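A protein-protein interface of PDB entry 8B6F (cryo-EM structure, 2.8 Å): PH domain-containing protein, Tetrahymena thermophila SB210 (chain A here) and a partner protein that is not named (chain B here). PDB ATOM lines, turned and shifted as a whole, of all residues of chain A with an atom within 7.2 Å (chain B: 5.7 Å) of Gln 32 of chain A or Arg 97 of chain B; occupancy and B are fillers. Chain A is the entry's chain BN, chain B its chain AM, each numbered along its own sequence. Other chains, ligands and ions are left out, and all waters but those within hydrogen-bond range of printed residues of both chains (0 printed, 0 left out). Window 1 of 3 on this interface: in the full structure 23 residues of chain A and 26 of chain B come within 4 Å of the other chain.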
ATOM      1  N   PHE A   5       8.354  19.917  10.220  1.00  0.00           N
ATOM      2  CA  PHE A   5       6.978  19.478  10.046  1.00  0.00           C
ATOM      3  C   PHE A   5       6.909  18.264   9.130  1.00  0.00           C
ATOM      4  O   PHE A   5       7.557  18.214   8.082  1.00  0.00           O
ATOM      5  CB  PHE A   5       6.124  20.607   9.474  1.00  0.00           C
ATOM      6  CG  PHE A   5       4.749  20.169   9.062  1.00  0.00           C
ATOM      7  CD1 PHE A   5       3.781  19.894  10.014  1.00  0.00           C
ATOM      8  CD2 PHE A   5       4.422  20.036   7.724  1.00  0.00           C
ATOM      9  CE1 PHE A   5       2.514  19.489   9.639  1.00  0.00           C
ATOM     10  CE2 PHE A   5       3.156  19.631   7.342  1.00  0.00           C
ATOM     11  CZ  PHE A   5       2.202  19.358   8.301  1.00  0.00           C
ATOM     12  N   GLU A   6       6.114  17.279   9.538  1.00  0.00           N
ATOM     13  CA  GLU A   6       5.859  16.085   8.748  1.00  0.00           C
ATOM     14  C   GLU A   6       4.356  15.905   8.624  1.00  0.00           C
ATOM     15  O   GLU A   6       3.640  15.945   9.628  1.00  0.00           O
ATOM     16  CB  GLU A   6       6.491  14.847   9.389  1.00  0.00           C
ATOM     17  CG  GLU A   6       6.263  13.562   8.605  1.00  0.00           C
ATOM     18  CD  GLU A   6       6.787  12.339   9.330  1.00  0.00           C
ATOM     19  OE1 GLU A   6       7.270  12.488  10.471  1.00  0.00           O
ATOM     20  OE2 GLU A   6       6.714  11.231   8.759  1.00  0.00           O
ATOM     21  N   ASN A   7       3.883  15.713   7.395  1.00  0.00           N
ATOM     22  CA  ASN A   7       2.465  15.478   7.138  1.00  0.00           C
ATOM     23  C   ASN A   7       2.229  13.975   7.215  1.00  0.00           C
ATOM     24  O   ASN A   7       2.430  13.251   6.238  1.00  0.00           O
ATOM     25  CB  ASN A   7       2.062  16.049   5.785  1.00  0.00           C
ATOM     26  CG  ASN A   7       0.563  16.184   5.633  1.00  0.00           C
ATOM     27  OD1 ASN A   7      -0.199  15.338   6.098  1.00  0.00           O
ATOM     28  ND2 ASN A   7       0.129  17.259   4.986  1.00  0.00           N
ATOM     29  N   VAL A   8       1.801  13.502   8.386  1.00  0.00           N
ATOM     30  CA  VAL A   8       1.651  12.066   8.599  1.00  0.00           C
ATOM     31  C   VAL A   8       0.609  11.491   7.649  1.00  0.00           C
ATOM     32  O   VAL A   8       0.748  10.366   7.157  1.00  0.00           O
ATOM     33  CB  VAL A   8       1.297  11.779  10.069  1.00  0.00           C
ATOM     34  CG1 VAL A   8       1.133  10.286  10.302  1.00  0.00           C
ATOM     35  CG2 VAL A   8       2.364  12.347  10.992  1.00  0.00           C
ATOM     36  N   LEU A   9      -0.457  12.247   7.383  1.00  0.00           N
ATOM     37  CA  LEU A   9      -1.503  11.750   6.498  1.00  0.00           C
ATOM     38  C   LEU A   9      -0.963  11.499   5.096  1.00  0.00           C
ATOM     39  O   LEU A   9      -1.304  10.492   4.463  1.00  0.00           O
ATOM     40  CB  LEU A   9      -2.669  12.737   6.457  1.00  0.00           C
ATOM     41  CG  LEU A   9      -3.860  12.326   5.589  1.00  0.00           C
ATOM     42  CD1 LEU A   9      -4.470  11.023   6.080  1.00  0.00           C
ATOM     43  CD2 LEU A   9      -4.899  13.426   5.565  1.00  0.00           C
ATOM     44  N   LEU A  10      -0.120  12.398   4.595  1.00  0.00           N
ATOM     45  CA  LEU A  10       0.459  12.265   3.267  1.00  0.00           C
ATOM     46  C   LEU A  10       1.759  11.474   3.265  1.00  0.00           C
ATOM     47  O   LEU A  10       2.379  11.332   2.207  1.00  0.00           O
ATOM     48  CB  LEU A  10       0.701  13.650   2.657  1.00  0.00           C
ATOM     49  CG  LEU A  10      -0.536  14.535   2.480  1.00  0.00           C
ATOM     50  CD1 LEU A  10      -0.148  15.903   1.943  1.00  0.00           C
ATOM     51  CD2 LEU A  10      -1.553  13.879   1.565  1.00  0.00           C
ATOM     52  N   ILE A  26      -4.755   9.221  13.402  1.00  0.00           N
ATOM     53  CA  ILE A  26      -5.648   9.829  14.383  1.00  0.00           C
ATOM     54  C   ILE A  26      -4.898  10.849  15.229  1.00  0.00           C
ATOM     55  O   ILE A  26      -5.393  11.956  15.474  1.00  0.00           O
ATOM     56  CB  ILE A  26      -6.304   8.739  15.251  1.00  0.00           C
ATOM     57  CG1 ILE A  26      -7.283   7.917  14.413  1.00  0.00           C
ATOM     58  CG2 ILE A  26      -7.028   9.357  16.442  1.00  0.00           C
ATOM     59  CD1 ILE A  26      -7.752   6.650  15.085  1.00  0.00           C
ATOM     60  N   ASN A  27      -3.695  10.501  15.688  1.00  0.00           N
ATOM     61  CA  ASN A  27      -2.929  11.434  16.507  1.00  0.00           C
ATOM     62  C   ASN A  27      -2.573  12.687  15.720  1.00  0.00           C
ATOM     63  O   ASN A  27      -2.673  13.805  16.235  1.00  0.00           O
ATOM     64  CB  ASN A  27      -1.665  10.761  17.036  1.00  0.00           C
ATOM     65  CG  ASN A  27      -1.968   9.599  17.955  1.00  0.00           C
ATOM     66  OD1 ASN A  27      -3.019   9.553  18.588  1.00  0.00           O
ATOM     67  ND2 ASN A  27      -1.041   8.654  18.037  1.00  0.00           N
ATOM     68  N   TYR A  28      -2.150  12.516  14.466  1.00  0.00           N
ATOM     69  CA  TYR A  28      -1.829  13.669  13.633  1.00  0.00           C
ATOM     70  C   TYR A  28      -3.056  14.542  13.416  1.00  0.00           C
ATOM     71  O   TYR A  28      -2.972  15.774  13.485  1.00  0.00           O
ATOM     72  CB  TYR A  28      -1.251  13.194  12.301  1.00  0.00           C
ATOM     73  CG  TYR A  28      -1.177  14.263  11.237  1.00  0.00           C
ATOM     74  CD1 TYR A  28      -0.246  15.289  11.318  1.00  0.00           C
ATOM     75  CD2 TYR A  28      -2.023  14.229  10.137  1.00  0.00           C
ATOM     76  CE1 TYR A  28      -0.172  16.261  10.343  1.00  0.00           C
ATOM     77  CE2 TYR A  28      -1.956  15.195   9.157  1.00  0.00           C
ATOM     78  CZ  TYR A  28      -1.028  16.206   9.265  1.00  0.00           C
ATOM     79  OH  TYR A  28      -0.961  17.172   8.288  1.00  0.00           O
ATOM     80  N   ALA A  29      -4.208  13.923  13.159  1.00  0.00           N
ATOM     81  CA  ALA A  29      -5.437  14.689  12.988  1.00  0.00           C
ATOM     82  C   ALA A  29      -5.786  15.464  14.251  1.00  0.00           C
ATOM     83  O   ALA A  29      -6.178  16.634  14.181  1.00  0.00           O
ATOM     84  CB  ALA A  29      -6.583  13.756  12.599  1.00  0.00           C
ATOM     85  N   LEU A  30      -5.646  14.831  15.417  1.00  0.00           N
ATOM     86  CA  LEU A  30      -5.948  15.519  16.668  1.00  0.00           C
ATOM     87  C   LEU A  30      -5.039  16.722  16.868  1.00  0.00           C
ATOM     88  O   LEU A  30      -5.499  17.796  17.274  1.00  0.00           O
ATOM     89  CB  LEU A  30      -5.818  14.551  17.844  1.00  0.00           C
ATOM     90  CG  LEU A  30      -6.864  13.436  17.927  1.00  0.00           C
ATOM     91  CD1 LEU A  30      -6.514  12.465  19.036  1.00  0.00           C
ATOM     92  CD2 LEU A  30      -8.259  13.999  18.137  1.00  0.00           C
ATOM     93  N   LEU A  31      -3.744  16.566  16.594  1.00  0.00           N
ATOM     94  CA  LEU A  31      -2.816  17.675  16.779  1.00  0.00           C
ATOM     95  C   LEU A  31      -3.143  18.828  15.838  1.00  0.00           C
ATOM     96  O   LEU A  31      -3.167  19.993  16.248  1.00  0.00           O
ATOM     97  CB  LEU A  31      -1.383  17.191  16.564  1.00  0.00           C
ATOM     98  CG  LEU A  31      -0.281  18.233  16.759  1.00  0.00           C
ATOM     99  CD1 LEU A  31      -0.341  18.854  18.145  1.00  0.00           C
ATOM    100  CD2 LEU A  31       1.080  17.603  16.514  1.00  0.00           C
ATOM    101  N   GLN A  32      -3.398  18.519  14.566  1.00  0.00           N
ATOM    102  CA  GLN A  32      -3.721  19.568  13.605  1.00  0.00           C
ATOM    103  C   GLN A  32      -5.037  20.248  13.954  1.00  0.00           C
ATOM    104  O   GLN A  32      -5.170  21.470  13.813  1.00  0.00           O
ATOM    105  CB  GLN A  32      -3.767  18.991  12.192  1.00  0.00           C
ATOM    106  CG  GLN A  32      -2.448  18.399  11.730  1.00  0.00           C
ATOM    107  CD  GLN A  32      -1.325  19.416  11.721  1.00  0.00           C
ATOM    108  OE1 GLN A  32      -1.542  20.595  11.449  1.00  0.00           O
ATOM    109  NE2 GLN A  32      -0.117  18.966  12.030  1.00  0.00           N
ATOM    110  N   ASP A  33      -6.020  19.475  14.417  1.00  0.00           N
ATOM    111  CA  ASP A  33      -7.288  20.060  14.836  1.00  0.00           C
ATOM    112  C   ASP A  33      -7.097  20.987  16.027  1.00  0.00           C
ATOM    113  O   ASP A  33      -7.737  22.040  16.111  1.00  0.00           O
ATOM    114  CB  ASP A  33      -8.289  18.957  15.176  1.00  0.00           C
ATOM    115  CG  ASP A  33      -8.652  18.112  13.975  1.00  0.00           C
ATOM    116  OD1 ASP A  33      -8.697  18.660  12.854  1.00  0.00           O
ATOM    117  OD2 ASP A  33      -8.896  16.900  14.150  1.00  0.00           O
ATOM    118  N   ALA A  34      -6.225  20.611  16.962  1.00  0.00           N
ATOM    119  CA  ALA A  34      -5.937  21.493  18.086  1.00  0.00           C
ATOM    120  C   ALA A  34      -5.312  22.800  17.616  1.00  0.00           C
ATOM    121  O   ALA A  34      -5.667  23.878  18.106  1.00  0.00           O
ATOM    122  CB  ALA A  34      -5.021  20.790  19.083  1.00  0.00           C
ATOM    123  N   LYS A  35      -4.372  22.728  16.672  1.00  0.00           N
ATOM    124  CA  LYS A  35      -3.773  23.949  16.144  1.00  0.00           C
ATOM    125  C   LYS A  35      -4.826  24.828  15.484  1.00  0.00           C
ATOM    126  O   LYS A  35      -4.858  26.044  15.702  1.00  0.00           O
ATOM    127  CB  LYS A  35      -2.665  23.606  15.151  1.00  0.00           C
ATOM    128  CG  LYS A  35      -1.479  22.885  15.763  1.00  0.00           C
ATOM    129  CD  LYS A  35      -0.420  22.598  14.711  1.00  0.00           C
ATOM    130  CE  LYS A  35       0.769  21.862  15.301  1.00  0.00           C
ATOM    131  NZ  LYS A  35       1.767  21.511  14.255  1.00  0.00           N
ATOM    132  N   GLN A  36      -5.700  24.230  14.672  1.00  0.00           N
ATOM    133  CA  GLN A  36      -6.751  25.001  14.016  1.00  0.00           C
ATOM    134  C   GLN A  36      -7.685  25.618  15.044  1.00  0.00           C
ATOM    135  O   GLN A  36      -8.105  26.772  14.904  1.00  0.00           O
ATOM    136  CB  GLN A  36      -7.533  24.111  13.052  1.00  0.00           C
ATOM    137  CG  GLN A  36      -8.662  24.828  12.326  1.00  0.00           C
ATOM    138  CD  GLN A  36      -9.489  23.887  11.481  1.00  0.00           C
ATOM    139  OE1 GLN A  36      -9.281  22.676  11.497  1.00  0.00           O
ATOM    140  NE2 GLN A  36     -10.436  24.440  10.736  1.00  0.00           N
ATOM    141  N   ARG A  37      -8.017  24.860  16.086  1.00  0.00           N
ATOM    142  CA  ARG A  37      -8.852  25.383  17.159  1.00  0.00           C
ATOM    143  C   ARG A  37      -8.206  26.599  17.805  1.00  0.00           C
ATOM    144  O   ARG A  37      -8.875  27.605  18.066  1.00  0.00           O
ATOM    145  CB  ARG A  37      -9.082  24.286  18.194  1.00  0.00           C
ATOM    146  CG  ARG A  37     -10.451  24.272  18.826  1.00  0.00           C
ATOM    147  CD  ARG A  37     -10.519  23.128  19.810  1.00  0.00           C
ATOM    148  NE  ARG A  37     -10.339  21.841  19.149  1.00  0.00           N
ATOM    149  CZ  ARG A  37      -9.901  20.742  19.747  1.00  0.00           C
ATOM    150  NH1 ARG A  37      -9.565  20.738  21.027  1.00  0.00           N
ATOM    151  NH2 ARG A  37      -9.789  19.621  19.042  1.00  0.00           N
ATOM    152  N   SER A  38      -6.904  26.521  18.080  1.00  0.00           N
ATOM    153  CA  SER A  38      -6.204  27.657  18.665  1.00  0.00           C
ATOM    154  C   SER A  38      -6.262  28.876  17.752  1.00  0.00           C
ATOM    155  O   SER A  38      -6.513  29.993  18.215  1.00  0.00           O
ATOM    156  CB  SER A  38      -4.753  27.273  18.951  1.00  0.00           C
ATOM    157  OG  SER A  38      -4.026  28.369  19.475  1.00  0.00           O
ATOM    158  N   ARG A  39      -6.030  28.684  16.452  1.00  0.00           N
ATOM    159  CA  ARG A  39      -6.036  29.813  15.526  1.00  0.00           C
ATOM    160  C   ARG A  39      -7.407  30.476  15.471  1.00  0.00           C
ATOM    161  O   ARG A  39      -7.521  31.703  15.557  1.00  0.00           O
ATOM    162  CB  ARG A  39      -5.608  29.355  14.133  1.00  0.00           C
ATOM    163  CG  ARG A  39      -4.140  28.973  14.024  1.00  0.00           C
ATOM    164  CD  ARG A  39      -3.734  28.763  12.574  1.00  0.00           C
ATOM    165  NE  ARG A  39      -4.482  27.680  11.946  1.00  0.00           N
ATOM    166  CZ  ARG A  39      -4.123  26.404  11.966  1.00  0.00           C
ATOM    167  NH1 ARG A  39      -3.023  26.003  12.581  1.00  0.00           N
ATOM    168  NH2 ARG A  39      -4.887  25.506  11.352  1.00  0.00           N
ATOM    169  N   ALA B  74     -11.746  24.766   5.741  1.00  0.00           N
ATOM    170  CA  ALA B  74     -10.445  24.110   5.820  1.00  0.00           C
ATOM    171  C   ALA B  74     -10.517  22.779   5.083  1.00  0.00           C
ATOM    172  O   ALA B  74     -10.929  21.763   5.643  1.00  0.00           O
ATOM    173  CB  ALA B  74     -10.035  23.914   7.274  1.00  0.00           C
ATOM    174  N   VAL B  75     -10.111  22.791   3.818  1.00  0.00           N
ATOM    175  CA  VAL B  75     -10.001  21.592   2.999  1.00  0.00           C
ATOM    176  C   VAL B  75      -8.557  21.479   2.538  1.00  0.00           C
ATOM    177  O   VAL B  75      -7.927  22.485   2.196  1.00  0.00           O
ATOM    178  CB  VAL B  75     -10.966  21.632   1.794  1.00  0.00           C
ATOM    179  CG1 VAL B  75     -10.779  20.409   0.909  1.00  0.00           C
ATOM    180  CG2 VAL B  75     -12.403  21.728   2.269  1.00  0.00           C
ATOM    181  N   TYR B  76      -8.036  20.255   2.527  1.00  0.00           N
ATOM    182  CA  TYR B  76      -6.655  19.995   2.141  1.00  0.00           C
ATOM    183  C   TYR B  76      -6.630  18.805   1.197  1.00  0.00           C
ATOM    184  O   TYR B  76      -6.997  17.694   1.591  1.00  0.00           O
ATOM    185  CB  TYR B  76      -5.785  19.721   3.372  1.00  0.00           C
ATOM    186  CG  TYR B  76      -5.797  20.848   4.374  1.00  0.00           C
ATOM    187  CD1 TYR B  76      -6.763  20.906   5.367  1.00  0.00           C
ATOM    188  CD2 TYR B  76      -4.846  21.854   4.325  1.00  0.00           C
ATOM    189  CE1 TYR B  76      -6.783  21.935   6.281  1.00  0.00           C
ATOM    190  CE2 TYR B  76      -4.856  22.888   5.236  1.00  0.00           C
ATOM    191  CZ  TYR B  76      -5.828  22.922   6.212  1.00  0.00           C
ATOM    192  OH  TYR B  76      -5.844  23.949   7.122  1.00  0.00           O
ATOM    193  N   ALA B  95     -11.829  20.634   9.764  1.00  0.00           N
ATOM    194  CA  ALA B  95     -11.055  20.481   8.544  1.00  0.00           C
ATOM    195  C   ALA B  95     -11.416  19.189   7.820  1.00  0.00           C
ATOM    196  O   ALA B  95     -11.987  18.260   8.393  1.00  0.00           O
ATOM    197  CB  ALA B  95      -9.558  20.497   8.854  1.00  0.00           C
ATOM    198  N   ILE B  96     -11.079  19.149   6.534  1.00  0.00           N
ATOM    199  CA  ILE B  96     -11.194  17.952   5.712  1.00  0.00           C
ATOM    200  C   ILE B  96      -9.848  17.752   5.035  1.00  0.00           C
ATOM    201  O   ILE B  96      -9.362  18.651   4.338  1.00  0.00           O
ATOM    202  CB  ILE B  96     -12.321  18.063   4.670  1.00  0.00           C
ATOM    203  CG1 ILE B  96     -13.674  18.199   5.372  1.00  0.00           C
ATOM    204  CG2 ILE B  96     -12.323  16.843   3.752  1.00  0.00           C
ATOM    205  CD1 ILE B  96     -14.834  18.470   4.437  1.00  0.00           C
ATOM    206  N   ARG B  97      -9.248  16.585   5.236  1.00  0.00           N
ATOM    207  CA  ARG B  97      -7.933  16.271   4.697  1.00  0.00           C
ATOM    208  C   ARG B  97      -8.030  15.064   3.782  1.00  0.00           C
ATOM    209  O   ARG B  97      -8.675  14.069   4.124  1.00  0.00           O
ATOM    210  CB  ARG B  97      -6.932  16.011   5.822  1.00  0.00           C
ATOM    211  CG  ARG B  97      -6.845  17.145   6.820  1.00  0.00           C
ATOM    212  CD  ARG B  97      -5.894  16.823   7.954  1.00  0.00           C
ATOM    213  NE  ARG B  97      -5.810  17.930   8.897  1.00  0.00           N
ATOM    214  CZ  ARG B  97      -6.665  18.145   9.887  1.00  0.00           C
ATOM    215  NH1 ARG B  97      -7.683  17.335  10.108  1.00  0.00           N
ATOM    216  NH2 ARG B  97      -6.494  19.202  10.674  1.00  0.00           N
ATOM    217  N   VAL B  98      -7.387  15.157   2.620  1.00  0.00           N
ATOM    218  CA  VAL B  98      -7.432  14.109   1.614  1.00  0.00           C
ATOM    219  C   VAL B  98      -6.005  13.771   1.196  1.00  0.00           C
ATOM    220  O   VAL B  98      -5.091  14.590   1.306  1.00  0.00           O
ATOM    221  CB  VAL B  98      -8.280  14.539   0.399  1.00  0.00           C
ATOM    222  CG1 VAL B  98      -8.520  13.383  -0.507  1.00  0.00           C
ATOM    223  CG2 VAL B  98      -9.608  15.124   0.851  1.00  0.00           C
ATOM    224  N   GLY B  99      -5.824  12.546   0.706  1.00  0.00           N
ATOM    225  CA  GLY B  99      -4.508  12.023   0.406  1.00  0.00           C
ATOM    226  C   GLY B  99      -4.026  12.365  -0.991  1.00  0.00           C
ATOM    227  O   GLY B  99      -4.649  13.121  -1.737  1.00  0.00           O
ATOM    228  N   SER B 123     -12.719  15.640  12.402  1.00  0.00           N
ATOM    229  CA  SER B 123     -12.401  16.005  11.035  1.00  0.00           C
ATOM    230  C   SER B 123     -12.337  14.753  10.173  1.00  0.00           C
ATOM    231  O   SER B 123     -12.053  13.657  10.663  1.00  0.00           O
ATOM    232  CB  SER B 123     -11.066  16.742  10.973  1.00  0.00           C
ATOM    233  OG  SER B 123     -10.037  15.918  11.490  1.00  0.00           O
ATOM    234  N   THR B 124     -12.610  14.923   8.884  1.00  0.00           N
ATOM    235  CA  THR B 124     -12.553  13.821   7.935  1.00  0.00           C
ATOM    236  C   THR B 124     -11.124  13.663   7.434  1.00  0.00           C
ATOM    237  O   THR B 124     -10.525  14.620   6.937  1.00  0.00           O
ATOM    238  CB  THR B 124     -13.501  14.063   6.760  1.00  0.00           C
ATOM    239  OG1 THR B 124     -14.812  14.360   7.255  1.00  0.00           O
ATOM    240  CG2 THR B 124     -13.572  12.833   5.868  1.00  0.00           C
ATOM    241  N   ASN B 125     -10.581  12.457   7.575  1.00  0.00           N
ATOM    242  CA  ASN B 125      -9.233  12.143   7.126  1.00  0.00           C
ATOM    243  C   ASN B 125      -9.291  10.924   6.223  1.00  0.00           C
ATOM    244  O   ASN B 125      -9.843   9.889   6.610  1.00  0.00           O
ATOM    245  CB  ASN B 125      -8.303  11.887   8.314  1.00  0.00           C
ATOM    246  CG  ASN B 125      -8.248  13.059   9.270  1.00  0.00           C
ATOM    247  OD1 ASN B 125      -7.449  13.977   9.099  1.00  0.00           O
ATOM    248  ND2 ASN B 125      -9.100  13.033  10.287  1.00  0.00           N
ATOM    249  N   ILE B 126      -8.719  11.041   5.027  1.00  0.00           N
ATOM    250  CA  ILE B 126      -8.807  10.007   4.006  1.00  0.00           C
ATOM    251  C   ILE B 126      -7.401   9.634   3.561  1.00  0.00           C
ATOM    252  O   ILE B 126      -6.522  10.495   3.457  1.00  0.00           O
ATOM    253  CB  ILE B 126      -9.665  10.474   2.810  1.00  0.00           C
ATOM    254  CG1 ILE B 126     -11.057  10.886   3.302  1.00  0.00           C
ATOM    255  CG2 ILE B 126      -9.772   9.376   1.765  1.00  0.00           C
ATOM    256  CD1 ILE B 126     -11.962  11.449   2.227  1.00  0.00           C
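Ile 26 of chain A touches none of the printed residues of chain B.
Leu 30 of chain A touches none of the printed residues of chain B.
Of the printed residues of chain B, Gln 32 of chain A touches Arg 97 (3.1 Å).
Of the printed residues of chain B, Asp 33 of chain A touches Arg 97 (3.1 Å) and Ser 123 (3.1 Å).
Of the printed residues of chain A, Ala 95 of chain B touches Gln 36 (3.4 Å).
Of chain A, only Leu 9 (3.3 Å), Gln 32 (3.1 Å) and Asp 33 (3.1 Å) come within 4 Å of Arg 97 of chain B.
Printed residues of chain A within 4 Å of Ser 123 of chain B: Asp 33.
Of the printed residues of chain A, Asn 125 of chain B touches Ala 29.
Printed residues of chain A within 4 Å of Ile 126 of chain B: Leu 9.
The nearest residue of chain A that does not touch Arg 97 of chain B is Ala 29 of chain A (4.4 Å).
Of the 20 printed residues of chain A, 6 touch a printed residue of chain B.
Hydrophobic or aromatic side chains of chain A within 4 Å of the printed part of chain B: Leu 9, Leu 10 and Ala 29.
Of the 12 printed residues of chain B, 8 touch a printed residue of chain A.
Among the printed residues, Asp or Glu carboxylates within 4 Å of a Lys or Arg side-chain nitrogen of the other chain: Asp 33 of chain A with Arg 97 of chain B.
The backbone carbonyl oxygen (O) of Ala 74 of chain B lies within hydrogen-bond range of the backbone NH (N) of Ile 96 of chain B, at 2.8 Å.
The backbone carbonyl oxygen (O) of Tyr 76 of chain B is in hydrogen-bond range of the backbone NH (N) of Val 98 of chain B.
The guanidinium group (NH1) of Arg 97 of chain B sits at hydrogen-bond distance from the side-chain hydroxyl (OG) of Ser 123 of chain B, 3.1 Å away.
O of Arg 97 of chain B sits at hydrogen-bond distance from N of Ile 126 of chain B (3.2 Å).
OD1 of Asn 7 of chain A sits at hydrogen-bond distance from N of Leu 10 of chain A (3.3 Å).
The side-chain carboxylate of Asp 33 of chain A sits close to the backbone carbonyl oxygen of Ala 29 of chain A (2.7 Å).
Arg 97 of chain B touches Leu 9 of chain A.
CD1 of Leu 9 of chain A touches O of Ile 126 of chain B, at 3.4 Å.
Leu 10 of chain A touches Val 98 of chain B (CD2 to O, 3.6 Å).
Gly 99 of chain B touches Leu 10 of chain A (CA to CD2, 3.7 Å).
Ala 29 of chain A touches Asn 125 of chain B (CB to ND2, 3.5 Å).
Arg 97 of chain B touches Gln 32 of chain A.
NE2 of Gln 36 of chain A touches CB of Ala 74 of chain B (3.5 Å).
Gln 36 of chain A touches Ala 95 of chain B.
The guanidinium group (NH2) of Arg 97 of chain B is in salt-bridge range of the side-chain carboxylate (OD1) of Asp 33 of chain A (3.1 Å).
OG of Ser 123 of chain B is in hydrogen-bond range of OD2 of Asp 33 of chain A, at 3.1 Å.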
